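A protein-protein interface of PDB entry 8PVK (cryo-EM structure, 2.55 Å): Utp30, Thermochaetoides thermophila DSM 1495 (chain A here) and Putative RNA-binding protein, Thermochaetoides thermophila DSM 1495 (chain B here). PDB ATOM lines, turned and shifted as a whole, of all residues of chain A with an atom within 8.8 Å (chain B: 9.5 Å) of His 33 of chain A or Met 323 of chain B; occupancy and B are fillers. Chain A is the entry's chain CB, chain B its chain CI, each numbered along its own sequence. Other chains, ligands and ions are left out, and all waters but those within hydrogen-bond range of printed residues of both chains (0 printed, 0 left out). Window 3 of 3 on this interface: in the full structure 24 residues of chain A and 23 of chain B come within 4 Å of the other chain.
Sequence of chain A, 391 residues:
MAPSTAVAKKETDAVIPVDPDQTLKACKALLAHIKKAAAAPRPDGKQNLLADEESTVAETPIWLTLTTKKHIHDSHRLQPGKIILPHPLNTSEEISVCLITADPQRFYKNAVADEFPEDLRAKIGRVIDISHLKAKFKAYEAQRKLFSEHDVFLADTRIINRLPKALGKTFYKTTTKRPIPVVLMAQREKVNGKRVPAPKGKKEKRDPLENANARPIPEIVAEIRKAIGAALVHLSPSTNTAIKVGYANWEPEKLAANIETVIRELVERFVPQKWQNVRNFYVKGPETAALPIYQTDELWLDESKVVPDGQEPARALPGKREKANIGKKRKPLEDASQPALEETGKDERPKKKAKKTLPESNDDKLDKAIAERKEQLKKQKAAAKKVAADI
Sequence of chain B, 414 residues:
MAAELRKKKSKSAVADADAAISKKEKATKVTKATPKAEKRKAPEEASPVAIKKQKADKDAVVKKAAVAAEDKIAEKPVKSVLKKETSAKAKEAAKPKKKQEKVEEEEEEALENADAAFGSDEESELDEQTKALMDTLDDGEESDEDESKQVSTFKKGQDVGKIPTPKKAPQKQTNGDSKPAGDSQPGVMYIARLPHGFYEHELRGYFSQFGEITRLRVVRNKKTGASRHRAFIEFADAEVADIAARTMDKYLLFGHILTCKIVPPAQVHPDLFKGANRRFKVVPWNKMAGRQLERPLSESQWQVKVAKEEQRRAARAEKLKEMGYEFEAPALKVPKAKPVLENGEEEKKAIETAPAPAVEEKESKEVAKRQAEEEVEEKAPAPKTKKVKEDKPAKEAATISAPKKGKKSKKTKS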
ATOM      1  N   LYS A  25      24.469  15.128 -17.799  1.00  0.00           N
ATOM      2  CA  LYS A  25      25.371  16.232 -18.105  1.00  0.00           C
ATOM      3  C   LYS A  25      24.846  17.555 -17.549  1.00  0.00           C
ATOM      4  O   LYS A  25      25.644  18.449 -17.242  1.00  0.00           O
ATOM      5  CB  LYS A  25      25.634  16.295 -19.616  1.00  0.00           C
ATOM      6  CG  LYS A  25      24.472  16.719 -20.489  1.00  0.00           C
ATOM      7  CD  LYS A  25      24.821  16.576 -21.970  1.00  0.00           C
ATOM      8  CE  LYS A  25      25.904  17.548 -22.413  1.00  0.00           C
ATOM      9  NZ  LYS A  25      25.452  18.962 -22.373  1.00  0.00           N
ATOM     10  N   ALA A  26      23.527  17.676 -17.353  1.00  0.00           N
ATOM     11  CA  ALA A  26      22.980  18.840 -16.658  1.00  0.00           C
ATOM     12  C   ALA A  26      23.412  18.876 -15.200  1.00  0.00           C
ATOM     13  O   ALA A  26      23.794  19.936 -14.688  1.00  0.00           O
ATOM     14  CB  ALA A  26      21.457  18.844 -16.750  1.00  0.00           C
ATOM     15  N   CYS A  27      23.344  17.732 -14.512  1.00  0.00           N
ATOM     16  CA  CYS A  27      23.833  17.679 -13.134  1.00  0.00           C
ATOM     17  C   CYS A  27      25.330  17.953 -13.062  1.00  0.00           C
ATOM     18  O   CYS A  27      25.787  18.663 -12.160  1.00  0.00           O
ATOM     19  CB  CYS A  27      23.505  16.338 -12.473  1.00  0.00           C
ATOM     20  SG  CYS A  27      21.825  15.733 -12.695  1.00  0.00           S
ATOM     21  N   LYS A  28      26.106  17.409 -14.009  1.00  0.00           N
ATOM     22  CA  LYS A  28      27.546  17.669 -14.026  1.00  0.00           C
ATOM     23  C   LYS A  28      27.851  19.154 -14.214  1.00  0.00           C
ATOM     24  O   LYS A  28      28.660  19.728 -13.471  1.00  0.00           O
ATOM     25  CB  LYS A  28      28.219  16.846 -15.125  1.00  0.00           C
ATOM     26  CG  LYS A  28      28.416  15.381 -14.777  1.00  0.00           C
ATOM     27  CD  LYS A  28      29.205  14.660 -15.858  1.00  0.00           C
ATOM     28  CE  LYS A  28      29.666  13.291 -15.386  1.00  0.00           C
ATOM     29  NZ  LYS A  28      28.528  12.364 -15.152  1.00  0.00           N
ATOM     30  N   ALA A  29      27.190  19.796 -15.185  1.00  0.00           N
ATOM     31  CA  ALA A  29      27.412  21.217 -15.433  1.00  0.00           C
ATOM     32  C   ALA A  29      26.958  22.070 -14.255  1.00  0.00           C
ATOM     33  O   ALA A  29      27.641  23.032 -13.884  1.00  0.00           O
ATOM     34  CB  ALA A  29      26.692  21.643 -16.712  1.00  0.00           C
ATOM     35  N   LEU A  30      25.817  21.726 -13.646  1.00  0.00           N
ATOM     36  CA  LEU A  30      25.316  22.506 -12.520  1.00  0.00           C
ATOM     37  C   LEU A  30      26.226  22.382 -11.304  1.00  0.00           C
ATOM     38  O   LEU A  30      26.485  23.376 -10.616  1.00  0.00           O
ATOM     39  CB  LEU A  30      23.892  22.074 -12.170  1.00  0.00           C
ATOM     40  CG  LEU A  30      23.237  22.872 -11.042  1.00  0.00           C
ATOM     41  CD1 LEU A  30      23.097  24.332 -11.440  1.00  0.00           C
ATOM     42  CD2 LEU A  30      21.889  22.286 -10.673  1.00  0.00           C
ATOM     43  N   LEU A  31      26.728  21.174 -11.026  1.00  0.00           N
ATOM     44  CA  LEU A  31      27.633  21.005  -9.894  1.00  0.00           C
ATOM     45  C   LEU A  31      28.963  21.710 -10.136  1.00  0.00           C
ATOM     46  O   LEU A  31      29.538  22.293  -9.205  1.00  0.00           O
ATOM     47  CB  LEU A  31      27.856  19.521  -9.604  1.00  0.00           C
ATOM     48  CG  LEU A  31      26.651  18.773  -9.029  1.00  0.00           C
ATOM     49  CD1 LEU A  31      26.999  17.324  -8.711  1.00  0.00           C
ATOM     50  CD2 LEU A  31      26.096  19.487  -7.814  1.00  0.00           C
ATOM     51  N   ALA A  32      29.470  21.667 -11.375  1.00  0.00           N
ATOM     52  CA  ALA A  32      30.695  22.398 -11.694  1.00  0.00           C
ATOM     53  C   ALA A  32      30.500  23.900 -11.530  1.00  0.00           C
ATOM     54  O   ALA A  32      31.374  24.592 -10.988  1.00  0.00           O
ATOM     55  CB  ALA A  32      31.150  22.066 -13.115  1.00  0.00           C
ATOM     56  N   HIS A  33      29.347  24.415 -11.971  1.00  0.00           N
ATOM     57  CA  HIS A  33      29.025  25.827 -11.789  1.00  0.00           C
ATOM     58  C   HIS A  33      28.929  26.191 -10.313  1.00  0.00           C
ATOM     59  O   HIS A  33      29.413  27.250  -9.897  1.00  0.00           O
ATOM     60  CB  HIS A  33      27.714  26.150 -12.502  1.00  0.00           C
ATOM     61  CG  HIS A  33      27.229  27.552 -12.291  1.00  0.00           C
ATOM     62  ND1 HIS A  33      27.559  28.589 -13.135  1.00  0.00           N
ATOM     63  CD2 HIS A  33      26.426  28.083 -11.339  1.00  0.00           C
ATOM     64  CE1 HIS A  33      26.988  29.701 -12.709  1.00  0.00           C
ATOM     65  NE2 HIS A  33      26.296  29.422 -11.620  1.00  0.00           N
ATOM     66  N   ILE A  34      28.311  25.318  -9.511  1.00  0.00           N
ATOM     67  CA  ILE A  34      28.156  25.577  -8.081  1.00  0.00           C
ATOM     68  C   ILE A  34      29.517  25.629  -7.397  1.00  0.00           C
ATOM     69  O   ILE A  34      29.792  26.531  -6.593  1.00  0.00           O
ATOM     70  CB  ILE A  34      27.235  24.517  -7.445  1.00  0.00           C
ATOM     71  CG1 ILE A  34      25.769  24.832  -7.754  1.00  0.00           C
ATOM     72  CG2 ILE A  34      27.453  24.419  -5.937  1.00  0.00           C
ATOM     73  CD1 ILE A  34      24.783  23.886  -7.096  1.00  0.00           C
ATOM     74  N   LYS A  35      30.401  24.680  -7.726  1.00  0.00           N
ATOM     75  CA  LYS A  35      31.726  24.681  -7.112  1.00  0.00           C
ATOM     76  C   LYS A  35      32.558  25.882  -7.552  1.00  0.00           C
ATOM     77  O   LYS A  35      33.251  26.489  -6.724  1.00  0.00           O
ATOM     78  CB  LYS A  35      32.469  23.375  -7.398  1.00  0.00           C
ATOM     79  CG  LYS A  35      31.817  22.137  -6.792  1.00  0.00           C
ATOM     80  CD  LYS A  35      32.650  20.884  -7.046  1.00  0.00           C
ATOM     81  CE  LYS A  35      32.637  20.445  -8.499  1.00  0.00           C
ATOM     82  NZ  LYS A  35      31.293  19.993  -8.935  1.00  0.00           N
ATOM     83  N   LYS A  36      32.500  26.264  -8.835  1.00  0.00           N
ATOM     84  CA  LYS A  36      33.319  27.399  -9.258  1.00  0.00           C
ATOM     85  C   LYS A  36      32.752  28.718  -8.743  1.00  0.00           C
ATOM     86  O   LYS A  36      33.503  29.686  -8.572  1.00  0.00           O
ATOM     87  CB  LYS A  36      33.492  27.414 -10.786  1.00  0.00           C
ATOM     88  CG  LYS A  36      32.252  27.627 -11.667  1.00  0.00           C
ATOM     89  CD  LYS A  36      31.983  29.101 -11.985  1.00  0.00           C
ATOM     90  CE  LYS A  36      30.820  29.265 -12.943  1.00  0.00           C
ATOM     91  NZ  LYS A  36      30.539  30.697 -13.239  1.00  0.00           N
ATOM     92  N   ALA A  37      31.443  28.779  -8.489  1.00  0.00           N
ATOM     93  CA  ALA A  37      30.864  29.968  -7.877  1.00  0.00           C
ATOM     94  C   ALA A  37      31.196  30.052  -6.392  1.00  0.00           C
ATOM     95  O   ALA A  37      31.459  31.142  -5.873  1.00  0.00           O
ATOM     96  CB  ALA A  37      29.349  29.985  -8.089  1.00  0.00           C
ATOM     97  N   ALA A  38      31.185  28.913  -5.693  1.00  0.00           N
ATOM     98  CA  ALA A  38      31.506  28.912  -4.271  1.00  0.00           C
ATOM     99  C   ALA A  38      32.997  29.070  -4.013  1.00  0.00           C
ATOM    100  O   ALA A  38      33.380  29.470  -2.907  1.00  0.00           O
ATOM    101  CB  ALA A  38      30.998  27.626  -3.619  1.00  0.00           C
ATOM    102  N   ALA A  39      33.845  28.754  -4.996  1.00  0.00           N
ATOM    103  CA  ALA A  39      35.278  28.960  -4.827  1.00  0.00           C
ATOM    104  C   ALA A  39      35.635  30.441  -4.782  1.00  0.00           C
ATOM    105  O   ALA A  39      36.566  30.831  -4.069  1.00  0.00           O
ATOM    106  CB  ALA A  39      36.046  28.264  -5.949  1.00  0.00           C
ATOM    107  N   ALA A  40      34.913  31.273  -5.526  1.00  0.00           N
ATOM    108  CA  ALA A  40      35.175  32.707  -5.547  1.00  0.00           C
ATOM    109  C   ALA A  40      34.665  33.378  -4.275  1.00  0.00           C
ATOM    110  O   ALA A  40      33.877  32.797  -3.529  1.00  0.00           O
ATOM    111  CB  ALA A  40      34.540  33.343  -6.773  1.00  0.00           C
ATOM    112  N   VAL A  57      29.158  25.011  -0.335  1.00  0.00           N
ATOM    113  CA  VAL A  57      28.683  23.975  -1.254  1.00  0.00           C
ATOM    114  C   VAL A  57      27.630  23.107  -0.572  1.00  0.00           C
ATOM    115  O   VAL A  57      26.597  22.770  -1.165  1.00  0.00           O
ATOM    116  CB  VAL A  57      29.869  23.141  -1.777  1.00  0.00           C
ATOM    117  CG1 VAL A  57      29.388  21.892  -2.495  1.00  0.00           C
ATOM    118  CG2 VAL A  57      30.720  23.975  -2.721  1.00  0.00           C
ATOM    119  N   ALA A 248      24.342  19.691  -3.329  1.00  0.00           N
ATOM    120  CA  ALA A 248      25.495  19.855  -4.205  1.00  0.00           C
ATOM    121  C   ALA A 248      26.586  18.822  -3.952  1.00  0.00           C
ATOM    122  O   ALA A 248      27.342  18.503  -4.876  1.00  0.00           O
ATOM    123  CB  ALA A 248      26.067  21.265  -4.059  1.00  0.00           C
ATOM    124  N   VAL A 283      16.470  22.192 -14.281  1.00  0.00           N
ATOM    125  CA  VAL A 283      17.232  21.899 -13.071  1.00  0.00           C
ATOM    126  C   VAL A 283      18.008  23.154 -12.701  1.00  0.00           C
ATOM    127  O   VAL A 283      18.630  23.778 -13.568  1.00  0.00           O
ATOM    128  CB  VAL A 283      18.176  20.697 -13.265  1.00  0.00           C
ATOM    129  CG1 VAL A 283      18.964  20.421 -11.998  1.00  0.00           C
ATOM    130  CG2 VAL A 283      17.387  19.463 -13.653  1.00  0.00           C
ATOM    131  N   LYS A 284      17.954  23.542 -11.427  1.00  0.00           N
ATOM    132  CA  LYS A 284      18.582  24.792 -11.026  1.00  0.00           C
ATOM    133  C   LYS A 284      19.012  24.726  -9.569  1.00  0.00           C
ATOM    134  O   LYS A 284      18.714  23.770  -8.849  1.00  0.00           O
ATOM    135  CB  LYS A 284      17.640  25.981 -11.243  1.00  0.00           C
ATOM    136  CG  LYS A 284      16.393  25.948 -10.380  1.00  0.00           C
ATOM    137  CD  LYS A 284      15.548  27.193 -10.589  1.00  0.00           C
ATOM    138  CE  LYS A 284      16.263  28.426 -10.072  1.00  0.00           C
ATOM    139  NZ  LYS A 284      15.355  29.594  -9.948  1.00  0.00           N
ATOM    140  N   GLY A 285      19.746  25.756  -9.155  1.00  0.00           N
ATOM    141  CA  GLY A 285      20.093  25.955  -7.770  1.00  0.00           C
ATOM    142  C   GLY A 285      19.411  27.193  -7.224  1.00  0.00           C
ATOM    143  O   GLY A 285      18.609  27.833  -7.910  1.00  0.00           O
ATOM    144  N   PRO A 286      19.697  27.540  -5.966  1.00  0.00           N
ATOM    145  CA  PRO A 286      19.109  28.762  -5.390  1.00  0.00           C
ATOM    146  C   PRO A 286      19.526  30.043  -6.097  1.00  0.00           C
ATOM    147  O   PRO A 286      18.736  30.992  -6.154  1.00  0.00           O
ATOM    148  CB  PRO A 286      19.606  28.736  -3.937  1.00  0.00           C
ATOM    149  CG  PRO A 286      19.941  27.305  -3.673  1.00  0.00           C
ATOM    150  CD  PRO A 286      20.465  26.776  -4.971  1.00  0.00           C
ATOM    151  N   GLU A 287      20.742  30.097  -6.640  1.00  0.00           N
ATOM    152  CA  GLU A 287      21.235  31.289  -7.313  1.00  0.00           C
ATOM    153  C   GLU A 287      21.633  31.048  -8.763  1.00  0.00           C
ATOM    154  O   GLU A 287      21.864  32.020  -9.492  1.00  0.00           O
ATOM    155  CB  GLU A 287      22.435  31.872  -6.548  1.00  0.00           C
ATOM    156  CG  GLU A 287      22.588  33.385  -6.658  1.00  0.00           C
ATOM    157  CD  GLU A 287      21.509  34.140  -5.905  1.00  0.00           C
ATOM    158  OE1 GLU A 287      20.974  33.593  -4.919  1.00  0.00           O
ATOM    159  OE2 GLU A 287      21.198  35.283  -6.300  1.00  0.00           O
ATOM    160  N   THR A 288      21.711  29.797  -9.205  1.00  0.00           N
ATOM    161  CA  THR A 288      22.111  29.490 -10.568  1.00  0.00           C
ATOM    162  C   THR A 288      20.949  29.723 -11.532  1.00  0.00           C
ATOM    163  O   THR A 288      19.829  30.055 -11.136  1.00  0.00           O
ATOM    164  CB  THR A 288      22.605  28.048 -10.663  1.00  0.00           C
ATOM    165  OG1 THR A 288      21.481  27.164 -10.738  1.00  0.00           O
ATOM    166  CG2 THR A 288      23.439  27.691  -9.443  1.00  0.00           C
ATOM    167  N   ALA A 289      21.224  29.546 -12.822  1.00  0.00           N
ATOM    168  CA  ALA A 289      20.196  29.631 -13.843  1.00  0.00           C
ATOM    169  C   ALA A 289      19.515  28.272 -14.001  1.00  0.00           C
ATOM    170  O   ALA A 289      19.846  27.299 -13.319  1.00  0.00           O
ATOM    171  CB  ALA A 289      20.792  30.113 -15.164  1.00  0.00           C
ATOM    172  N   ALA A 290      18.556  28.199 -14.918  1.00  0.00           N
ATOM    173  CA  ALA A 290      17.775  26.990 -15.139  1.00  0.00           C
ATOM    174  C   ALA A 290      18.308  26.260 -16.366  1.00  0.00           C
ATOM    175  O   ALA A 290      18.361  26.834 -17.459  1.00  0.00           O
ATOM    176  CB  ALA A 290      16.294  27.325 -15.314  1.00  0.00           C
ATOM    177  N   LEU A 291      18.697  24.998 -16.184  1.00  0.00           N
ATOM    178  CA  LEU A 291      19.163  24.165 -17.279  1.00  0.00           C
ATOM    179  C   LEU A 291      18.007  23.316 -17.774  1.00  0.00           C
ATOM    180  O   LEU A 291      17.463  22.522 -16.990  1.00  0.00           O
ATOM    181  CB  LEU A 291      20.313  23.273 -16.828  1.00  0.00           C
ATOM    182  CG  LEU A 291      21.380  23.887 -15.919  1.00  0.00           C
ATOM    183  CD1 LEU A 291      22.435  22.854 -15.577  1.00  0.00           C
ATOM    184  CD2 LEU A 291      22.019  25.095 -16.575  1.00  0.00           C
ATOM    185  N   PRO A 292      17.577  23.466 -19.026  1.00  0.00           N
ATOM    186  CA  PRO A 292      16.447  22.671 -19.520  1.00  0.00           C
ATOM    187  C   PRO A 292      16.794  21.196 -19.658  1.00  0.00           C
ATOM    188  O   PRO A 292      17.941  20.826 -19.917  1.00  0.00           O
ATOM    189  CB  PRO A 292      16.139  23.299 -20.884  1.00  0.00           C
ATOM    190  CG  PRO A 292      17.392  24.010 -21.273  1.00  0.00           C
ATOM    191  CD  PRO A 292      18.008  24.484 -19.997  1.00  0.00           C
ATOM    192  N   ARG B 316      17.597  32.117 -23.817  1.00  0.00           N
ATOM    193  CA  ARG B 316      18.078  31.123 -22.862  1.00  0.00           C
ATOM    194  C   ARG B 316      19.273  30.348 -23.407  1.00  0.00           C
ATOM    195  O   ARG B 316      20.169  29.980 -22.642  1.00  0.00           O
ATOM    196  CB  ARG B 316      16.941  30.181 -22.464  1.00  0.00           C
ATOM    197  CG  ARG B 316      16.047  30.771 -21.383  1.00  0.00           C
ATOM    198  CD  ARG B 316      14.926  29.833 -20.981  1.00  0.00           C
ATOM    199  NE  ARG B 316      13.881  29.767 -21.995  1.00  0.00           N
ATOM    200  CZ  ARG B 316      12.783  29.034 -21.890  1.00  0.00           C
ATOM    201  NH1 ARG B 316      12.549  28.291 -20.822  1.00  0.00           N
ATOM    202  NH2 ARG B 316      11.893  29.050 -22.879  1.00  0.00           N
ATOM    203  N   ALA B 317      19.330  30.128 -24.723  1.00  0.00           N
ATOM    204  CA  ALA B 317      20.477  29.448 -25.319  1.00  0.00           C
ATOM    205  C   ALA B 317      21.741  30.297 -25.235  1.00  0.00           C
ATOM    206  O   ALA B 317      22.820  29.783 -24.914  1.00  0.00           O
ATOM    207  CB  ALA B 317      20.172  29.080 -26.771  1.00  0.00           C
ATOM    208  N   GLU B 318      21.636  31.597 -25.519  1.00  0.00           N
ATOM    209  CA  GLU B 318      22.809  32.451 -25.388  1.00  0.00           C
ATOM    210  C   GLU B 318      23.179  32.713 -23.933  1.00  0.00           C
ATOM    211  O   GLU B 318      24.333  33.061 -23.661  1.00  0.00           O
ATOM    212  CB  GLU B 318      22.616  33.771 -26.155  1.00  0.00           C
ATOM    213  CG  GLU B 318      21.467  34.668 -25.713  1.00  0.00           C
ATOM    214  CD  GLU B 318      21.831  35.601 -24.572  1.00  0.00           C
ATOM    215  OE1 GLU B 318      23.039  35.836 -24.357  1.00  0.00           O
ATOM    216  OE2 GLU B 318      20.909  36.097 -23.892  1.00  0.00           O
ATOM    217  N   LYS B 319      22.238  32.554 -22.997  1.00  0.00           N
ATOM    218  CA  LYS B 319      22.619  32.515 -21.588  1.00  0.00           C
ATOM    219  C   LYS B 319      23.305  31.201 -21.230  1.00  0.00           C
ATOM    220  O   LYS B 319      24.155  31.172 -20.333  1.00  0.00           O
ATOM    221  CB  LYS B 319      21.395  32.734 -20.699  1.00  0.00           C
ATOM    222  CG  LYS B 319      20.850  34.153 -20.727  1.00  0.00           C
ATOM    223  CD  LYS B 319      21.833  35.130 -20.106  1.00  0.00           C
ATOM    224  CE  LYS B 319      21.898  34.959 -18.597  1.00  0.00           C
ATOM    225  NZ  LYS B 319      22.786  35.971 -17.962  1.00  0.00           N
ATOM    226  N   LEU B 320      22.945  30.109 -21.904  1.00  0.00           N
ATOM    227  CA  LEU B 320      23.572  28.816 -21.660  1.00  0.00           C
ATOM    228  C   LEU B 320      24.913  28.654 -22.361  1.00  0.00           C
ATOM    229  O   LEU B 320      25.620  27.680 -22.077  1.00  0.00           O
ATOM    230  CB  LEU B 320      22.640  27.683 -22.098  1.00  0.00           C
ATOM    231  CG  LEU B 320      21.446  27.360 -21.200  1.00  0.00           C
ATOM    232  CD1 LEU B 320      20.459  26.477 -21.942  1.00  0.00           C
ATOM    233  CD2 LEU B 320      21.906  26.696 -19.918  1.00  0.00           C
ATOM    234  N   LYS B 321      25.251  29.549 -23.295  1.00  0.00           N
ATOM    235  CA  LYS B 321      26.534  29.454 -23.995  1.00  0.00           C
ATOM    236  C   LYS B 321      27.714  29.559 -23.031  1.00  0.00           C
ATOM    237  O   LYS B 321      28.625  28.723 -23.062  1.00  0.00           O
ATOM    238  CB  LYS B 321      26.637  30.533 -25.075  1.00  0.00           C
ATOM    239  CG  LYS B 321      25.707  30.351 -26.267  1.00  0.00           C
ATOM    240  CD  LYS B 321      26.042  29.110 -27.082  1.00  0.00           C
ATOM    241  CE  LYS B 321      24.910  28.093 -27.034  1.00  0.00           C
ATOM    242  NZ  LYS B 321      25.092  27.003 -28.031  1.00  0.00           N
ATOM    243  N   GLU B 322      27.717  30.571 -22.161  1.00  0.00           N
ATOM    244  CA  GLU B 322      28.793  30.698 -21.184  1.00  0.00           C
ATOM    245  C   GLU B 322      28.570  29.835 -19.950  1.00  0.00           C
ATOM    246  O   GLU B 322      29.463  29.749 -19.100  1.00  0.00           O
ATOM    247  CB  GLU B 322      28.975  32.162 -20.767  1.00  0.00           C
ATOM    248  CG  GLU B 322      28.014  32.661 -19.695  1.00  0.00           C
ATOM    249  CD  GLU B 322      26.653  33.044 -20.240  1.00  0.00           C
ATOM    250  OE1 GLU B 322      26.466  33.014 -21.474  1.00  0.00           O
ATOM    251  OE2 GLU B 322      25.769  33.388 -19.427  1.00  0.00           O
ATOM    252  N   MET B 323      27.403  29.197 -19.838  1.00  0.00           N
ATOM    253  CA  MET B 323      27.134  28.243 -18.769  1.00  0.00           C
ATOM    254  C   MET B 323      27.989  26.987 -18.894  1.00  0.00           C
ATOM    255  O   MET B 323      28.213  26.295 -17.893  1.00  0.00           O
ATOM    256  CB  MET B 323      25.643  27.885 -18.798  1.00  0.00           C
ATOM    257  CG  MET B 323      25.103  27.018 -17.673  1.00  0.00           C
ATOM    258  SD  MET B 323      25.142  27.796 -16.054  1.00  0.00           S
ATOM    259  CE  MET B 323      25.146  26.340 -15.019  1.00  0.00           C
ATOM    260  N   GLY B 324      28.497  26.695 -20.089  1.00  0.00           N
ATOM    261  CA  GLY B 324      29.133  25.421 -20.340  1.00  0.00           C
ATOM    262  C   GLY B 324      28.166  24.327 -20.719  1.00  0.00           C
ATOM    263  O   GLY B 324      28.550  23.154 -20.744  1.00  0.00           O
ATOM    264  N   TYR B 325      26.918  24.680 -21.017  1.00  0.00           N
ATOM    265  CA  TYR B 325      25.872  23.724 -21.348  1.00  0.00           C
ATOM    266  C   TYR B 325      25.387  23.912 -22.777  1.00  0.00           C
ATOM    267  O   TYR B 325      25.297  25.039 -23.274  1.00  0.00           O
ATOM    268  CB  TYR B 325      24.681  23.835 -20.391  1.00  0.00           C
ATOM    269  CG  TYR B 325      23.950  22.527 -20.253  1.00  0.00           C
ATOM    270  CD1 TYR B 325      24.625  21.372 -19.890  1.00  0.00           C
ATOM    271  CD2 TYR B 325      22.591  22.435 -20.529  1.00  0.00           C
ATOM    272  CE1 TYR B 325      23.968  20.171 -19.785  1.00  0.00           C
ATOM    273  CE2 TYR B 325      21.921  21.233 -20.424  1.00  0.00           C
ATOM    274  CZ  TYR B 325      22.617  20.104 -20.051  1.00  0.00           C
ATOM    275  OH  TYR B 325      21.963  18.900 -19.946  1.00  0.00           O
ATOM    276  N   GLU B 326      25.075  22.793 -23.429  1.00  0.00           N
ATOM    277  CA  GLU B 326      24.535  22.783 -24.783  1.00  0.00           C
ATOM    278  C   GLU B 326      23.265  21.943 -24.782  1.00  0.00           C
ATOM    279  O   GLU B 326      23.314  20.739 -24.505  1.00  0.00           O
ATOM    280  CB  GLU B 326      25.557  22.232 -25.778  1.00  0.00           C
ATOM    281  CG  GLU B 326      26.791  23.106 -25.946  1.00  0.00           C
ATOM    282  CD  GLU B 326      26.483  24.443 -26.592  1.00  0.00           C
ATOM    283  OE1 GLU B 326      25.554  24.505 -27.425  1.00  0.00           O
ATOM    284  OE2 GLU B 326      27.168  25.434 -26.262  1.00  0.00           O
ATOM    285  N   PHE B 327      22.133  22.574 -25.084  1.00  0.00           N
ATOM    286  CA  PHE B 327      20.851  21.892 -25.200  1.00  0.00           C
ATOM    287  C   PHE B 327      20.307  22.069 -26.608  1.00  0.00           C
ATOM    288  O   PHE B 327      20.245  23.192 -27.118  1.00  0.00           O
ATOM    289  CB  PHE B 327      19.836  22.418 -24.183  1.00  0.00           C
ATOM    290  CG  PHE B 327      18.626  21.539 -24.029  1.00  0.00           C
ATOM    291  CD1 PHE B 327      17.357  22.034 -24.291  1.00  0.00           C
ATOM    292  CD2 PHE B 327      18.755  20.216 -23.637  1.00  0.00           C
ATOM    293  CE1 PHE B 327      16.241  21.229 -24.157  1.00  0.00           C
ATOM    294  CE2 PHE B 327      17.642  19.406 -23.502  1.00  0.00           C
ATOM    295  CZ  PHE B 327      16.384  19.914 -23.762  1.00  0.00           C
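The backbone NH (N) of Ala 26 of chain A sits close to the side-chain hydroxyl (OH) of Tyr 325 of chain B, at 3.3 Å.
O of Val 283 of chain A lies within hydrogen-bond range of N of Leu 291 of chain A, 2.9 Å away.
O of Leu 320 of chain B lies within hydrogen-bond range of N of Tyr 325 of chain B, at 3.4 Å.
The side-chain amino group of Lys 321 of chain B lies within salt-bridge range of the side-chain carboxylate of Glu 326 of chain B.
Among the printed residues, pairs that only touch across the chains: Lys 25 of chain A with Tyr 325 of chain B, Lys 25 of chain A with Glu 326 of chain B, Ala 29 of chain A with Tyr 325 of chain B, His 33 of chain A with Met 323 of chain B, Leu 291 of chain A with Leu 320 of chain B, Leu 291 of chain A with Met 323 of chain B, Pro 292 of chain A with Leu 320 of chain B and Pro 292 of chain A with Phe 327 of chain B.
Printed residues of chain B within 4 Å of Lys 25 of chain A: Tyr 325 and Glu 326.
Cys 27 of chain A touches none of the printed residues of chain B.
No residue of chain B comes within 4 Å of Ala 32 of chain A.
His 33 of chain A touches just one residue of chain B: Met 323 (3.6 Å).
Of the printed residues of chain B, Leu 291 of chain A touches Leu 320 (3.7 Å) and Met 323 (3.7 Å).
Printed residues of chain B within 4 Å of Pro 292 of chain A: Leu 320 (3.7 Å) and Phe 327 (3.6 Å).
No residue of chain A comes within 4 Å of Glu 322 of chain B.
Met 323 of chain B touches just these residues of chain A: His 33 (3.6 Å) and Leu 291 (3.7 Å).
No residue of chain A comes within 4 Å of Gly 324 of chain B.
Of the printed residues of chain A, Tyr 325 of chain B touches Lys 25, Ala 26 and Ala 29.
Of the printed residues of chain A, Phe 327 of chain B touches Pro 292.
The nearest residue of chain B that does not touch His 33 of chain A is Glu 322 of chain B (6.4 Å).
The nearest residue of chain A that does not touch Met 323 of chain B is Ala 29 of chain A (4.3 Å).
Hydrophobic or aromatic side chains of chain B within 4 Å of the printed part of chain A: Leu 320, Met 323, Tyr 325 and Phe 327.
Hydrophobic or aromatic side chains of chain A within 4 Å of the printed part of chain B: Ala 26, Ala 29, His 33, Leu 291 and Pro 292.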
